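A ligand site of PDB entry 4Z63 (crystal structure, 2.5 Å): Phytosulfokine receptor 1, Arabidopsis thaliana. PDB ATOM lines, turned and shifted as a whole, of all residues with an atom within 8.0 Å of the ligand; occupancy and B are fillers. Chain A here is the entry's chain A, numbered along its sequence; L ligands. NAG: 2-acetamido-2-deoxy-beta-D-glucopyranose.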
ATOM      1  N   GLY A 170      19.411 -21.522   2.550  1.00  0.00           N
ATOM      2  CA  GLY A 170      19.062 -22.520   1.557  1.00  0.00           C
ATOM      3  C   GLY A 170      17.683 -23.131   1.746  1.00  0.00           C
ATOM      4  O   GLY A 170      17.189 -23.806   0.847  1.00  0.00           O
ATOM      5  N   VAL A 173      13.125 -21.503  -0.163  1.00  0.00           N
ATOM      6  CA  VAL A 173      13.256 -22.257  -1.384  1.00  0.00           C
ATOM      7  C   VAL A 173      12.943 -21.333  -2.565  1.00  0.00           C
ATOM      8  O   VAL A 173      13.448 -21.502  -3.667  1.00  0.00           O
ATOM      9  CB  VAL A 173      12.318 -23.515  -1.342  1.00  0.00           C
ATOM     10  CG1 VAL A 173      12.227 -24.185  -2.678  1.00  0.00           C
ATOM     11  CG2 VAL A 173      12.815 -24.528  -0.290  1.00  0.00           C
ATOM     12  N   GLU A 191      27.588 -23.929   2.050  1.00  0.00           N
ATOM     13  CA  GLU A 191      27.178 -24.687   0.860  1.00  0.00           C
ATOM     14  C   GLU A 191      25.643 -24.777   0.763  1.00  0.00           C
ATOM     15  O   GLU A 191      25.076 -25.077  -0.289  1.00  0.00           O
ATOM     16  CB  GLU A 191      27.819 -26.066   0.838  1.00  0.00           C
ATOM     17  CG  GLU A 191      27.378 -27.021   1.930  1.00  0.00           C
ATOM     18  CD  GLU A 191      28.145 -28.335   1.873  1.00  0.00           C
ATOM     19  OE1 GLU A 191      29.394 -28.283   1.832  1.00  0.00           O
ATOM     20  OE2 GLU A 191      27.488 -29.399   1.846  1.00  0.00           O
ATOM     21  N   ASP A 192      25.019 -24.482   1.882  1.00  0.00           N
ATOM     22  CA  ASP A 192      23.592 -24.265   2.039  1.00  0.00           C
ATOM     23  C   ASP A 192      23.052 -23.352   0.913  1.00  0.00           C
ATOM     24  O   ASP A 192      22.043 -23.658   0.262  1.00  0.00           O
ATOM     25  CB  ASP A 192      23.453 -23.584   3.403  1.00  0.00           C
ATOM     26  CG  ASP A 192      22.053 -23.113   3.709  1.00  0.00           C
ATOM     27  OD1 ASP A 192      21.713 -21.967   3.348  1.00  0.00           O
ATOM     28  OD2 ASP A 192      21.318 -23.870   4.361  1.00  0.00           O
ATOM     29  N   LEU A 193      23.746 -22.247   0.691  1.00  0.00           N
ATOM     30  CA  LEU A 193      23.313 -21.205  -0.239  1.00  0.00           C
ATOM     31  C   LEU A 193      23.126 -21.713  -1.674  1.00  0.00           C
ATOM     32  O   LEU A 193      22.284 -21.212  -2.396  1.00  0.00           O
ATOM     33  CB  LEU A 193      24.303 -20.042  -0.231  1.00  0.00           C
ATOM     34  CG  LEU A 193      23.981 -18.872  -1.162  1.00  0.00           C
ATOM     35  CD1 LEU A 193      22.769 -18.130  -0.697  1.00  0.00           C
ATOM     36  CD2 LEU A 193      25.143 -17.923  -1.249  1.00  0.00           C
ATOM     37  N   PHE A 194      23.907 -22.719  -2.055  1.00  0.00           N
ATOM     38  CA  PHE A 194      23.852 -23.261  -3.403  1.00  0.00           C
ATOM     39  C   PHE A 194      22.594 -24.090  -3.712  1.00  0.00           C
ATOM     40  O   PHE A 194      22.419 -24.572  -4.825  1.00  0.00           O
ATOM     41  CB  PHE A 194      25.132 -24.018  -3.722  1.00  0.00           C
ATOM     42  CG  PHE A 194      26.365 -23.206  -3.466  1.00  0.00           C
ATOM     43  CD1 PHE A 194      26.499 -21.948  -4.022  1.00  0.00           C
ATOM     44  CD2 PHE A 194      27.339 -23.658  -2.603  1.00  0.00           C
ATOM     45  CE1 PHE A 194      27.590 -21.188  -3.761  1.00  0.00           C
ATOM     46  CE2 PHE A 194      28.442 -22.890  -2.339  1.00  0.00           C
ATOM     47  CZ  PHE A 194      28.570 -21.660  -2.929  1.00  0.00           C
ATOM     48  N   HIS A 195      21.734 -24.271  -2.709  1.00  0.00           N
ATOM     49  CA  HIS A 195      20.414 -24.854  -2.950  1.00  0.00           C
ATOM     50  C   HIS A 195      19.406 -23.854  -3.531  1.00  0.00           C
ATOM     51  O   HIS A 195      18.306 -24.245  -3.893  1.00  0.00           O
ATOM     52  CB  HIS A 195      19.795 -25.458  -1.686  1.00  0.00           C
ATOM     53  CG  HIS A 195      20.604 -26.568  -1.078  1.00  0.00           C
ATOM     54  ND1 HIS A 195      21.776 -27.032  -1.635  1.00  0.00           N
ATOM     55  CD2 HIS A 195      20.411 -27.288   0.051  1.00  0.00           C
ATOM     56  CE1 HIS A 195      22.265 -27.996  -0.872  1.00  0.00           C
ATOM     57  NE2 HIS A 195      21.459 -28.167   0.160  1.00  0.00           N
ATOM     58  N   LEU A 196      19.733 -22.574  -3.621  1.00  0.00           N
ATOM     59  CA  LEU A 196      18.658 -21.681  -3.998  1.00  0.00           C
ATOM     60  C   LEU A 196      18.676 -21.547  -5.492  1.00  0.00           C
ATOM     61  O   LEU A 196      19.288 -20.652  -6.024  1.00  0.00           O
ATOM     62  CB  LEU A 196      18.890 -20.304  -3.380  1.00  0.00           C
ATOM     63  CG  LEU A 196      19.058 -20.276  -1.865  1.00  0.00           C
ATOM     64  CD1 LEU A 196      19.425 -18.900  -1.347  1.00  0.00           C
ATOM     65  CD2 LEU A 196      17.774 -20.726  -1.231  1.00  0.00           C
ATOM     66  N   LYS A 197      17.830 -22.316  -6.157  1.00  0.00           N
ATOM     67  CA  LYS A 197      17.893 -22.412  -7.611  1.00  0.00           C
ATOM     68  C   LYS A 197      17.055 -21.332  -8.288  1.00  0.00           C
ATOM     69  O   LYS A 197      17.064 -21.222  -9.517  1.00  0.00           O
ATOM     70  CB  LYS A 197      17.417 -23.795  -8.075  1.00  0.00           C
ATOM     71  CG  LYS A 197      18.486 -24.875  -8.075  1.00  0.00           C
ATOM     72  CD  LYS A 197      18.015 -26.075  -8.887  1.00  0.00           C
ATOM     73  CE  LYS A 197      19.128 -26.640  -9.764  1.00  0.00           C
ATOM     74  NZ  LYS A 197      19.555 -25.705 -10.855  1.00  0.00           N
ATOM     75  N   ARG A 198      16.291 -20.590  -7.497  1.00  0.00           N
ATOM     76  CA  ARG A 198      15.525 -19.474  -8.036  1.00  0.00           C
ATOM     77  C   ARG A 198      16.146 -18.088  -7.793  1.00  0.00           C
ATOM     78  O   ARG A 198      15.609 -17.077  -8.247  1.00  0.00           O
ATOM     79  CB  ARG A 198      14.066 -19.519  -7.561  1.00  0.00           C
ATOM     80  CG  ARG A 198      13.203 -20.512  -8.331  1.00  0.00           C
ATOM     81  CD  ARG A 198      12.213 -21.245  -7.414  1.00  0.00           C
ATOM     82  NE  ARG A 198      12.922 -22.045  -6.416  1.00  0.00           N
ATOM     83  CZ  ARG A 198      13.174 -23.349  -6.529  1.00  0.00           C
ATOM     84  NH1 ARG A 198      12.720 -24.037  -7.581  1.00  0.00           N
ATOM     85  NH2 ARG A 198      13.854 -23.969  -5.575  1.00  0.00           N
ATOM     86  N   SER A 214      32.926 -21.499  -4.584  1.00  0.00           N
ATOM     87  CA  SER A 214      32.702 -22.934  -4.841  1.00  0.00           C
ATOM     88  C   SER A 214      32.199 -23.248  -6.230  1.00  0.00           C
ATOM     89  O   SER A 214      31.478 -22.471  -6.845  1.00  0.00           O
ATOM     90  CB  SER A 214      31.746 -23.538  -3.819  1.00  0.00           C
ATOM     91  OG  SER A 214      31.477 -24.885  -4.163  1.00  0.00           O
ATOM     92  N   ARG A 215      32.545 -24.431  -6.715  1.00  0.00           N
ATOM     93  CA  ARG A 215      32.073 -24.888  -8.005  1.00  0.00           C
ATOM     94  C   ARG A 215      30.589 -25.202  -7.929  1.00  0.00           C
ATOM     95  O   ARG A 215      29.915 -25.274  -8.955  1.00  0.00           O
ATOM     96  CB  ARG A 215      32.876 -26.106  -8.445  1.00  0.00           C
ATOM     97  CG  ARG A 215      32.643 -26.548  -9.867  1.00  0.00           C
ATOM     98  CD  ARG A 215      33.863 -27.275 -10.409  1.00  0.00           C
ATOM     99  NE  ARG A 215      34.956 -26.349 -10.698  1.00  0.00           N
ATOM    100  CZ  ARG A 215      35.378 -26.054 -11.930  1.00  0.00           C
ATOM    101  NH1 ARG A 215      34.793 -26.623 -12.968  1.00  0.00           N
ATOM    102  NH2 ARG A 215      36.384 -25.180 -12.115  1.00  0.00           N
ATOM    103  N   GLU A 216      30.069 -25.357  -6.717  1.00  0.00           N
ATOM    104  CA  GLU A 216      28.655 -25.662  -6.528  1.00  0.00           C
ATOM    105  C   GLU A 216      27.761 -24.507  -6.982  1.00  0.00           C
ATOM    106  O   GLU A 216      26.550 -24.656  -7.113  1.00  0.00           O
ATOM    107  CB  GLU A 216      28.343 -26.025  -5.073  1.00  0.00           C
ATOM    108  CG  GLU A 216      28.952 -27.344  -4.591  1.00  0.00           C
ATOM    109  CD  GLU A 216      28.679 -28.528  -5.516  1.00  0.00           C
ATOM    110  OE1 GLU A 216      27.632 -28.530  -6.211  1.00  0.00           O
ATOM    111  OE2 GLU A 216      29.506 -29.465  -5.548  1.00  0.00           O
ATOM    112  N   ILE A 217      28.395 -23.368  -7.222  1.00  0.00           N
ATOM    113  CA  ILE A 217      27.691 -22.191  -7.694  1.00  0.00           C
ATOM    114  C   ILE A 217      27.023 -22.406  -9.059  1.00  0.00           C
ATOM    115  O   ILE A 217      26.119 -21.655  -9.450  1.00  0.00           O
ATOM    116  CB  ILE A 217      28.636 -20.974  -7.704  1.00  0.00           C
ATOM    117  CG1 ILE A 217      27.919 -19.725  -7.189  1.00  0.00           C
ATOM    118  CG2 ILE A 217      29.245 -20.743  -9.075  1.00  0.00           C
ATOM    119  CD1 ILE A 217      28.862 -18.587  -6.931  1.00  0.00           C
ATOM    120  N   ARG A 218      27.434 -23.447  -9.781  1.00  0.00           N
ATOM    121  CA  ARG A 218      26.780 -23.816 -11.023  1.00  0.00           C
ATOM    122  C   ARG A 218      25.347 -24.236 -10.765  1.00  0.00           C
ATOM    123  O   ARG A 218      24.535 -24.379 -11.679  1.00  0.00           O
ATOM    124  CB  ARG A 218      27.497 -24.985 -11.668  1.00  0.00           C
ATOM    125  CG  ARG A 218      27.436 -26.276 -10.871  1.00  0.00           C
ATOM    126  CD  ARG A 218      28.310 -27.278 -11.552  1.00  0.00           C
ATOM    127  NE  ARG A 218      28.805 -28.259 -10.614  1.00  0.00           N
ATOM    128  CZ  ARG A 218      28.298 -29.473 -10.493  1.00  0.00           C
ATOM    129  NH1 ARG A 218      27.285 -29.831 -11.277  1.00  0.00           N
ATOM    130  NH2 ARG A 218      28.797 -30.323  -9.610  1.00  0.00           N
ATOM    131  N   ASN A 219      25.026 -24.433  -9.497  1.00  0.00           N
ATOM    132  CA  ASN A 219      23.687 -24.864  -9.188  1.00  0.00           C
ATOM    133  C   ASN A 219      22.723 -23.706  -9.102  1.00  0.00           C
ATOM    134  O   ASN A 219      21.510 -23.924  -9.037  1.00  0.00           O
ATOM    135  CB  ASN A 219      23.658 -25.679  -7.900  1.00  0.00           C
ATOM    136  CG  ASN A 219      22.502 -26.626  -7.862  1.00  0.00           C
ATOM    137  OD1 ASN A 219      22.534 -27.710  -8.446  1.00  0.00           O
ATOM    138  ND2 ASN A 219      21.479 -26.243  -7.156  1.00  0.00           N
ATOM    139  N   LEU A 220      23.233 -22.476  -9.126  1.00  0.00           N
ATOM    140  CA  LEU A 220      22.288 -21.400  -9.046  1.00  0.00           C
ATOM    141  C   LEU A 220      22.080 -20.886 -10.436  1.00  0.00           C
ATOM    142  O   LEU A 220      22.606 -19.852 -10.810  1.00  0.00           O
ATOM    143  CB  LEU A 220      22.886 -20.275  -8.190  1.00  0.00           C
ATOM    144  CG  LEU A 220      23.370 -20.594  -6.776  1.00  0.00           C
ATOM    145  CD1 LEU A 220      24.157 -19.428  -6.185  1.00  0.00           C
ATOM    146  CD2 LEU A 220      22.213 -20.983  -5.840  1.00  0.00           C
ATOM    147  N   SER A 221      21.100 -21.457 -11.122  1.00  0.00           N
ATOM    148  CA  SER A 221      21.033 -21.315 -12.555  1.00  0.00           C
ATOM    149  C   SER A 221      20.174 -20.125 -12.945  1.00  0.00           C
ATOM    150  O   SER A 221      20.064 -19.805 -14.125  1.00  0.00           O
ATOM    151  CB  SER A 221      20.491 -22.601 -13.191  1.00  0.00           C
ATOM    152  OG  SER A 221      19.181 -22.871 -12.716  1.00  0.00           O
HETATM  153  C1  NAG L   1      20.637 -30.079  -3.814  1.00  0.00           C
HETATM  154  C2  NAG L   1      21.524 -29.305  -4.787  1.00  0.00           C
HETATM  155  C3  NAG L   1      20.940 -27.943  -4.995  1.00  0.00           C
HETATM  156  C4  NAG L   1      19.543 -28.191  -5.490  1.00  0.00           C
HETATM  157  C5  NAG L   1      18.760 -28.661  -4.271  1.00  0.00           C
HETATM  158  C6  NAG L   1      17.252 -28.596  -4.511  1.00  0.00           C
HETATM  159  C7  NAG L   1      23.893 -29.212  -4.989  1.00  0.00           C
HETATM  160  C8  NAG L   1      25.193 -28.833  -4.339  1.00  0.00           C
HETATM  161  N2  NAG L   1      22.826 -29.033  -4.231  1.00  0.00           N
HETATM  162  O4  NAG L   1      19.079 -26.996  -6.049  1.00  0.00           O
HETATM  163  O5  NAG L   1      19.217 -29.957  -3.872  1.00  0.00           O
HETATM  164  O6  NAG L   1      16.960 -28.239  -5.846  1.00  0.00           O
HETATM  165  O7  NAG L   1      23.809 -29.675  -6.129  1.00  0.00           O
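Merely in contact with the ligand: Phe 194 (3.7 Å), Lys 197 (3.0 Å) and Glu 216 (3.1 Å).
Hydrophobic or aromatic side chains within 4 Å of the ligand: His 195.
A ring nitrogen (ND1) of His 195 lies within hydrogen-bond range of a nitrogen (N2) of the ligand.
O4 of the ligand lies within hydrogen-bond range of ND2 of Asn 219.
N of Glu 216 lies within hydrogen-bond range of OG of Ser 214, at 3.0 Å.
ND2 of Asn 219 sits at hydrogen-bond distance from O of Phe 194 (3.0 Å).
The backbone carbonyl oxygen (O) of Asn 219 sits at hydrogen-bond distance from the side-chain amino group (NZ) of Lys 197.
The side-chain amino group (NZ) of Lys 197 lies within hydrogen-bond range of the side-chain hydroxyl (OG) of Ser 221, 3.4 Å away.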
